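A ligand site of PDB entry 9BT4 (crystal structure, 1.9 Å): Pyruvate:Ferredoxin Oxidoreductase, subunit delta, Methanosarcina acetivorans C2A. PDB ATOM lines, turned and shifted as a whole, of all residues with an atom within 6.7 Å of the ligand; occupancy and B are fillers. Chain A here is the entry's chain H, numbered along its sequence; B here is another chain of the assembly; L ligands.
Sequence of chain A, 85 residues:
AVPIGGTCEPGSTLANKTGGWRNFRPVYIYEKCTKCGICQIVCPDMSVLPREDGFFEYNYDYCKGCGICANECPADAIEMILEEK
Pro 26 touches the ligand (CG to S1, 3.7 Å). CD of Pro 44 touches S4 of the ligand, at 3.7 Å. CG2 of Val 48 touches S3 of the ligand, at 3.8 Å. Tyr 58 touches the ligand. CA of Gly 65 touches S1 of the ligand (3.6 Å). Hydrophobic or aromatic side chains that line the ligand: Pro 26, Pro 44, Val 48 and Tyr 58. 11 residues have an atom within 4 Å of the ligand: Pro 26, Cys 43, Pro 44, Val 48, Tyr 58, Cys 63, Lys 64, Gly 65, Cys 66, Gly 67 and Cys 69.
SG of Cys 43 sits close to N of Asp 45 (3.3 Å). SG of Cys 43 sits close to N of Ser 47 (3.3 Å). SG of Cys 43 sits close to N of Met 46. The backbone NH (N) of Gly 65 sits close to the side-chain sulfur (SG) of Cys 63 (3.3 Å). N of Cys 63 lies within hydrogen-bond range of OG of Ser 47 (3.3 Å). O of Cys 63 lies within hydrogen-bond range of NH1 of Arg 22 (2.9 Å). The side-chain sulfur (SG) of Cys 66 sits close to the backbone NH (N) of Ile 68, at 3.4 Å. OD2 of Asp 45 is in salt-bridge range of NZ of Lys 64 (2.7 Å).
The side-chain sulfur (SG) of Cys 43 is bound to an iron atom (FE1) of the ligand, at 2.2 Å. FE4 of the ligand is bound by SG of Cys 63 (2.3 Å). A sulfur (S4) of the ligand lies close to the backbone NH (N) of Cys 69 (3.6 Å). The side-chain sulfur (SG) of Cys 69 binds an iron atom (FE2) of the ligand (2.3 Å). A sulfur (S1) of the ligand sits close to the backbone NH of Cys 66 (3.4 Å). The side-chain sulfur (SG) of Cys 66 is bound to an iron atom (FE3) of the ligand, at 2.3 Å. N of Gly 67 sits close to S1 of the ligand (3.3 Å). N of Lys 64 sits close to S2 of the ligand (3.5 Å).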
ATOM      1  N   ARG A  22      31.012  29.088  35.300  1.00  0.00           N
ATOM      2  CA  ARG A  22      30.836  27.802  34.643  1.00  0.00           C
ATOM      3  C   ARG A  22      31.787  26.748  35.228  1.00  0.00           C
ATOM      4  O   ARG A  22      32.965  26.995  35.433  1.00  0.00           O
ATOM      5  CB  ARG A  22      31.104  27.883  33.139  1.00  0.00           C
ATOM      6  CG  ARG A  22      30.041  28.579  32.310  1.00  0.00           C
ATOM      7  CD  ARG A  22      30.198  28.249  30.830  1.00  0.00           C
ATOM      8  NE  ARG A  22      31.446  28.753  30.270  1.00  0.00           N
ATOM      9  CZ  ARG A  22      31.693  30.000  29.877  1.00  0.00           C
ATOM     10  NH1 ARG A  22      30.751  30.927  29.940  1.00  0.00           N
ATOM     11  NH2 ARG A  22      32.890  30.304  29.389  1.00  0.00           N
ATOM     12  N   PHE A  24      30.762  23.705  33.616  1.00  0.00           N
ATOM     13  CA  PHE A  24      30.528  23.069  32.331  1.00  0.00           C
ATOM     14  C   PHE A  24      30.126  24.141  31.321  1.00  0.00           C
ATOM     15  O   PHE A  24      29.604  25.191  31.696  1.00  0.00           O
ATOM     16  CB  PHE A  24      29.439  21.993  32.433  1.00  0.00           C
ATOM     17  CG  PHE A  24      29.811  20.820  33.332  1.00  0.00           C
ATOM     18  CD1 PHE A  24      30.459  19.704  32.824  1.00  0.00           C
ATOM     19  CD2 PHE A  24      29.487  20.835  34.690  1.00  0.00           C
ATOM     20  CE1 PHE A  24      30.803  18.639  33.646  1.00  0.00           C
ATOM     21  CE2 PHE A  24      29.831  19.770  35.512  1.00  0.00           C
ATOM     22  CZ  PHE A  24      30.478  18.672  34.987  1.00  0.00           C
ATOM     23  N   ARG A  25      30.370  23.865  30.033  1.00  0.00           N
ATOM     24  CA  ARG A  25      30.122  24.827  28.984  1.00  0.00           C
ATOM     25  C   ARG A  25      29.343  24.156  27.862  1.00  0.00           C
ATOM     26  O   ARG A  25      29.701  23.058  27.432  1.00  0.00           O
ATOM     27  CB  ARG A  25      31.463  25.397  28.519  1.00  0.00           C
ATOM     28  CG  ARG A  25      31.383  26.317  27.304  1.00  0.00           C
ATOM     29  CD  ARG A  25      32.699  27.009  27.003  1.00  0.00           C
ATOM     30  NE  ARG A  25      33.803  26.061  26.835  1.00  0.00           N
ATOM     31  CZ  ARG A  25      35.000  26.365  26.347  1.00  0.00           C
ATOM     32  NH1 ARG A  25      35.261  27.590  25.944  1.00  0.00           N
ATOM     33  NH2 ARG A  25      35.920  25.422  26.251  1.00  0.00           N
ATOM     34  N   PRO A  26      28.266  24.794  27.331  1.00  0.00           N
ATOM     35  CA  PRO A  26      27.532  24.250  26.185  1.00  0.00           C
ATOM     36  C   PRO A  26      28.278  24.526  24.893  1.00  0.00           C
ATOM     37  O   PRO A  26      28.934  25.560  24.751  1.00  0.00           O
ATOM     38  CB  PRO A  26      26.205  25.005  26.281  1.00  0.00           C
ATOM     39  CG  PRO A  26      26.601  26.372  26.786  1.00  0.00           C
ATOM     40  CD  PRO A  26      27.699  26.065  27.803  1.00  0.00           C
ATOM     41  N   TYR A  28      27.498  24.067  20.613  1.00  0.00           N
ATOM     42  CA  TYR A  28      26.575  23.722  19.540  1.00  0.00           C
ATOM     43  C   TYR A  28      27.229  22.711  18.604  1.00  0.00           C
ATOM     44  O   TYR A  28      28.374  22.870  18.207  1.00  0.00           O
ATOM     45  CB  TYR A  28      26.162  24.938  18.706  1.00  0.00           C
ATOM     46  CG  TYR A  28      25.102  25.818  19.346  1.00  0.00           C
ATOM     47  CD1 TYR A  28      23.775  25.401  19.424  1.00  0.00           C
ATOM     48  CD2 TYR A  28      25.418  27.074  19.849  1.00  0.00           C
ATOM     49  CE1 TYR A  28      22.798  26.189  20.008  1.00  0.00           C
ATOM     50  CE2 TYR A  28      24.442  27.882  20.430  1.00  0.00           C
ATOM     51  CZ  TYR A  28      23.136  27.434  20.507  1.00  0.00           C
ATOM     52  OH  TYR A  28      22.180  28.220  21.084  1.00  0.00           O
ATOM     53  N   CYS A  39      16.383  26.732  22.361  1.00  0.00           N
ATOM     54  CA  CYS A  39      17.510  27.058  23.228  1.00  0.00           C
ATOM     55  C   CYS A  39      17.517  28.544  23.577  1.00  0.00           C
ATOM     56  O   CYS A  39      17.903  28.904  24.695  1.00  0.00           O
ATOM     57  CB  CYS A  39      18.845  26.676  22.611  1.00  0.00           C
ATOM     58  SG  CYS A  39      19.039  27.120  20.862  1.00  0.00           S
ATOM     59  N   VAL A  42      14.840  29.209  26.353  1.00  0.00           N
ATOM     60  CA  VAL A  42      14.952  28.570  27.660  1.00  0.00           C
ATOM     61  C   VAL A  42      16.165  29.082  28.435  1.00  0.00           C
ATOM     62  O   VAL A  42      16.364  28.677  29.584  1.00  0.00           O
ATOM     63  CB  VAL A  42      14.959  27.031  27.579  1.00  0.00           C
ATOM     64  CG1 VAL A  42      13.620  26.476  27.115  1.00  0.00           C
ATOM     65  CG2 VAL A  42      16.100  26.497  26.725  1.00  0.00           C
ATOM     66  N   CYS A  43      16.993  29.948  27.826  1.00  0.00           N
ATOM     67  CA  CYS A  43      18.198  30.401  28.503  1.00  0.00           C
ATOM     68  C   CYS A  43      17.849  31.424  29.586  1.00  0.00           C
ATOM     69  O   CYS A  43      17.317  32.492  29.275  1.00  0.00           O
ATOM     70  CB  CYS A  43      19.198  31.051  27.552  1.00  0.00           C
ATOM     71  SG  CYS A  43      20.729  31.523  28.410  1.00  0.00           S
ATOM     72  N   PRO A  44      18.143  31.146  30.877  1.00  0.00           N
ATOM     73  CA  PRO A  44      17.857  32.088  31.967  1.00  0.00           C
ATOM     74  C   PRO A  44      18.722  33.345  31.891  1.00  0.00           C
ATOM     75  O   PRO A  44      18.420  34.349  32.538  1.00  0.00           O
ATOM     76  CB  PRO A  44      18.165  31.289  33.244  1.00  0.00           C
ATOM     77  CG  PRO A  44      18.257  29.843  32.786  1.00  0.00           C
ATOM     78  CD  PRO A  44      18.773  29.905  31.362  1.00  0.00           C
ATOM     79  N   ASP A  45      19.798  33.280  31.097  1.00  0.00           N
ATOM     80  CA  ASP A  45      20.837  34.284  31.158  1.00  0.00           C
ATOM     81  C   ASP A  45      20.988  35.030  29.837  1.00  0.00           C
ATOM     82  O   ASP A  45      21.951  35.756  29.648  1.00  0.00           O
ATOM     83  CB  ASP A  45      22.119  33.677  31.704  1.00  0.00           C
ATOM     84  CG  ASP A  45      22.097  33.473  33.221  1.00  0.00           C
ATOM     85  OD1 ASP A  45      21.746  32.357  33.655  1.00  0.00           O
ATOM     86  OD2 ASP A  45      22.418  34.441  33.927  1.00  0.00           O
ATOM     87  N   MET A  46      19.998  34.861  28.948  1.00  0.00           N
ATOM     88  CA  MET A  46      19.950  35.554  27.667  1.00  0.00           C
ATOM     89  C   MET A  46      21.303  35.482  26.965  1.00  0.00           C
ATOM     90  O   MET A  46      21.773  36.473  26.401  1.00  0.00           O
ATOM     91  CB  MET A  46      19.532  37.018  27.865  1.00  0.00           C
ATOM     92  CG  MET A  46      18.044  37.234  28.061  1.00  0.00           C
ATOM     93  SD  MET A  46      17.335  36.493  29.537  1.00  0.00           S
ATOM     94  CE  MET A  46      18.182  37.409  30.838  1.00  0.00           C
ATOM     95  N   SER A  47      21.910  34.290  26.988  1.00  0.00           N
ATOM     96  CA  SER A  47      23.248  34.076  26.456  1.00  0.00           C
ATOM     97  C   SER A  47      23.202  33.299  25.131  1.00  0.00           C
ATOM     98  O   SER A  47      24.241  32.899  24.620  1.00  0.00           O
ATOM     99  CB  SER A  47      24.122  33.385  27.465  1.00  0.00           C
ATOM    100  OG  SER A  47      24.351  34.233  28.575  1.00  0.00           O
ATOM    101  N   VAL A  48      21.987  33.078  24.613  1.00  0.00           N
ATOM    102  CA  VAL A  48      21.795  32.478  23.307  1.00  0.00           C
ATOM    103  C   VAL A  48      21.359  33.579  22.343  1.00  0.00           C
ATOM    104  O   VAL A  48      20.271  34.139  22.502  1.00  0.00           O
ATOM    105  CB  VAL A  48      20.783  31.316  23.331  1.00  0.00           C
ATOM    106  CG1 VAL A  48      20.472  30.802  21.931  1.00  0.00           C
ATOM    107  CG2 VAL A  48      21.226  30.171  24.224  1.00  0.00           C
ATOM    108  N   TYR A  58      26.435  31.214  21.285  1.00  0.00           N
ATOM    109  CA  TYR A  58      26.517  31.501  22.713  1.00  0.00           C
ATOM    110  C   TYR A  58      27.306  32.776  22.958  1.00  0.00           C
ATOM    111  O   TYR A  58      28.282  33.046  22.269  1.00  0.00           O
ATOM    112  CB  TYR A  58      27.185  30.333  23.436  1.00  0.00           C
ATOM    113  CG  TYR A  58      26.335  29.079  23.526  1.00  0.00           C
ATOM    114  CD1 TYR A  58      25.058  29.111  24.069  1.00  0.00           C
ATOM    115  CD2 TYR A  58      26.804  27.866  23.030  1.00  0.00           C
ATOM    116  CE1 TYR A  58      24.273  27.976  24.144  1.00  0.00           C
ATOM    117  CE2 TYR A  58      26.033  26.718  23.092  1.00  0.00           C
ATOM    118  CZ  TYR A  58      24.757  26.772  23.646  1.00  0.00           C
ATOM    119  OH  TYR A  58      23.993  25.645  23.712  1.00  0.00           O
ATOM    120  N   ASN A  59      26.848  33.550  23.950  1.00  0.00           N
ATOM    121  CA  ASN A  59      27.678  34.592  24.538  1.00  0.00           C
ATOM    122  C   ASN A  59      28.321  34.020  25.808  1.00  0.00           C
ATOM    123  O   ASN A  59      27.719  34.027  26.875  1.00  0.00           O
ATOM    124  CB  ASN A  59      26.904  35.895  24.726  1.00  0.00           C
ATOM    125  CG  ASN A  59      27.812  37.052  25.113  1.00  0.00           C
ATOM    126  OD1 ASN A  59      28.915  36.835  25.618  1.00  0.00           O
ATOM    127  ND2 ASN A  59      27.353  38.277  24.889  1.00  0.00           N
ATOM    128  N   TYR A  62      28.615  35.456  29.441  1.00  0.00           N
ATOM    129  CA  TYR A  62      27.545  35.444  30.429  1.00  0.00           C
ATOM    130  C   TYR A  62      27.062  34.024  30.747  1.00  0.00           C
ATOM    131  O   TYR A  62      26.563  33.792  31.849  1.00  0.00           O
ATOM    132  CB  TYR A  62      26.403  36.397  30.057  1.00  0.00           C
ATOM    133  CG  TYR A  62      26.894  37.824  29.832  1.00  0.00           C
ATOM    134  CD1 TYR A  62      27.243  38.632  30.897  1.00  0.00           C
ATOM    135  CD2 TYR A  62      27.049  38.322  28.548  1.00  0.00           C
ATOM    136  CE1 TYR A  62      27.718  39.921  30.697  1.00  0.00           C
ATOM    137  CE2 TYR A  62      27.517  39.607  28.326  1.00  0.00           C
ATOM    138  CZ  TYR A  62      27.859  40.407  29.400  1.00  0.00           C
ATOM    139  OH  TYR A  62      28.326  41.666  29.198  1.00  0.00           O
ATOM    140  N   CYS A  63      27.200  33.097  29.792  1.00  0.00           N
ATOM    141  CA  CYS A  63      26.674  31.746  29.983  1.00  0.00           C
ATOM    142  C   CYS A  63      27.190  31.164  31.298  1.00  0.00           C
ATOM    143  O   CYS A  63      28.394  31.164  31.547  1.00  0.00           O
ATOM    144  CB  CYS A  63      27.059  30.839  28.814  1.00  0.00           C
ATOM    145  SG  CYS A  63      26.684  29.087  29.105  1.00  0.00           S
ATOM    146  N   LYS A  64      26.262  30.654  32.123  1.00  0.00           N
ATOM    147  CA  LYS A  64      26.567  30.127  33.445  1.00  0.00           C
ATOM    148  C   LYS A  64      26.681  28.595  33.411  1.00  0.00           C
ATOM    149  O   LYS A  64      26.954  27.974  34.434  1.00  0.00           O
ATOM    150  CB  LYS A  64      25.517  30.570  34.480  1.00  0.00           C
ATOM    151  CG  LYS A  64      25.624  32.016  34.951  1.00  0.00           C
ATOM    152  CD  LYS A  64      24.397  32.479  35.746  1.00  0.00           C
ATOM    153  CE  LYS A  64      24.453  33.917  36.169  1.00  0.00           C
ATOM    154  NZ  LYS A  64      23.147  34.433  36.574  1.00  0.00           N
ATOM    155  N   GLY A  65      26.447  28.009  32.233  1.00  0.00           N
ATOM    156  CA  GLY A  65      26.661  26.591  31.992  1.00  0.00           C
ATOM    157  C   GLY A  65      25.707  25.712  32.805  1.00  0.00           C
ATOM    158  O   GLY A  65      26.106  24.660  33.308  1.00  0.00           O
ATOM    159  N   CYS A  66      24.447  26.139  32.888  1.00  0.00           N
ATOM    160  CA  CYS A  66      23.423  25.436  33.656  1.00  0.00           C
ATOM    161  C   CYS A  66      22.993  24.171  32.925  1.00  0.00           C
ATOM    162  O   CYS A  66      22.616  23.184  33.566  1.00  0.00           O
ATOM    163  CB  CYS A  66      22.228  26.372  33.863  1.00  0.00           C
ATOM    164  SG  CYS A  66      21.249  26.778  32.389  1.00  0.00           S
ATOM    165  N   GLY A  67      23.042  24.205  31.596  1.00  0.00           N
ATOM    166  CA  GLY A  67      22.775  23.032  30.768  1.00  0.00           C
ATOM    167  C   GLY A  67      21.300  22.858  30.438  1.00  0.00           C
ATOM    168  O   GLY A  67      20.902  21.785  29.988  1.00  0.00           O
ATOM    169  N   ILE A  68      20.480  23.911  30.642  1.00  0.00           N
ATOM    170  CA  ILE A  68      19.056  23.848  30.313  1.00  0.00           C
ATOM    171  C   ILE A  68      18.862  23.719  28.800  1.00  0.00           C
ATOM    172  O   ILE A  68      18.036  22.927  28.353  1.00  0.00           O
ATOM    173  CB  ILE A  68      18.262  25.039  30.887  1.00  0.00           C
ATOM    174  CG1 ILE A  68      18.085  24.938  32.401  1.00  0.00           C
ATOM    175  CG2 ILE A  68      16.902  25.164  30.200  1.00  0.00           C
ATOM    176  CD1 ILE A  68      17.368  26.117  33.028  1.00  0.00           C
ATOM    177  N   CYS A  69      19.590  24.537  28.028  1.00  0.00           N
ATOM    178  CA  CYS A  69      19.496  24.488  26.572  1.00  0.00           C
ATOM    179  C   CYS A  69      19.772  23.074  26.078  1.00  0.00           C
ATOM    180  O   CYS A  69      19.039  22.556  25.243  1.00  0.00           O
ATOM    181  CB  CYS A  69      20.418  25.519  25.926  1.00  0.00           C
ATOM    182  SG  CYS A  69      22.139  25.475  26.473  1.00  0.00           S
ATOM    183  N   ALA A  70      20.835  22.458  26.619  1.00  0.00           N
ATOM    184  CA  ALA A  70      21.247  21.116  26.247  1.00  0.00           C
ATOM    185  C   ALA A  70      20.182  20.088  26.621  1.00  0.00           C
ATOM    186  O   ALA A  70      19.974  19.117  25.900  1.00  0.00           O
ATOM    187  CB  ALA A  70      22.576  20.781  26.901  1.00  0.00           C
ATOM    188  N   ILE A  78      23.313  20.036  21.310  1.00  0.00           N
ATOM    189  CA  ILE A  78      24.141  20.766  22.256  1.00  0.00           C
ATOM    190  C   ILE A  78      24.840  19.763  23.165  1.00  0.00           C
ATOM    191  O   ILE A  78      24.209  18.875  23.718  1.00  0.00           O
ATOM    192  CB  ILE A  78      23.317  21.793  23.047  1.00  0.00           C
ATOM    193  CG1 ILE A  78      22.603  22.793  22.125  1.00  0.00           C
ATOM    194  CG2 ILE A  78      24.202  22.508  24.083  1.00  0.00           C
ATOM    195  CD1 ILE A  78      21.464  23.555  22.780  1.00  0.00           C
ATOM    196  N   MET A  80      27.492  19.389  26.553  1.00  0.00           N
ATOM    197  CA  MET A  80      28.107  20.026  27.705  1.00  0.00           C
ATOM    198  C   MET A  80      29.516  19.465  27.895  1.00  0.00           C
ATOM    199  O   MET A  80      29.685  18.252  28.056  1.00  0.00           O
ATOM    200  CB  MET A  80      27.284  19.799  28.981  1.00  0.00           C
ATOM    201  CG  MET A  80      25.848  20.337  28.938  1.00  0.00           C
ATOM    202  SD  MET A  80      25.713  22.088  28.551  1.00  0.00           S
ATOM    203  CE  MET A  80      26.495  22.864  29.971  1.00  0.00           C
ATOM    204  N   ALA B  18      22.660  29.329  38.499  1.00  0.00           N
ATOM    205  CA  ALA B  18      22.600  28.576  37.256  1.00  0.00           C
ATOM    206  C   ALA B  18      21.226  27.906  37.165  1.00  0.00           C
ATOM    207  O   ALA B  18      20.833  27.182  38.082  1.00  0.00           O
ATOM    208  CB  ALA B  18      23.726  27.558  37.208  1.00  0.00           C
ATOM    209  N   GLY B  19      20.496  28.218  36.087  1.00  0.00           N
ATOM    210  CA  GLY B  19      19.214  27.603  35.806  1.00  0.00           C
ATOM    211  C   GLY B  19      18.052  28.244  36.576  1.00  0.00           C
ATOM    212  O   GLY B  19      17.062  27.575  36.855  1.00  0.00           O
HETATM  213 FE1  LIG L   1      21.903  29.657  28.846  1.00  0.00          FE
HETATM  214 FE2  LIG L   1      22.608  27.171  27.902  1.00  0.00          FE
HETATM  215 FE3  LIG L   1      22.382  27.655  30.626  1.00  0.00          FE
HETATM  216 FE4  LIG L   1      24.452  28.706  29.155  1.00  0.00          FE
HETATM  217  S1  LIG L   1      24.065  26.523  29.531  1.00  0.00           S
HETATM  218  S2  LIG L   1      23.174  29.773  30.755  1.00  0.00           S
HETATM  219  S3  LIG L   1      23.393  29.157  27.192  1.00  0.00           S
HETATM  220  S4  LIG L   1      20.712  27.741  29.079  1.00  0.00           S
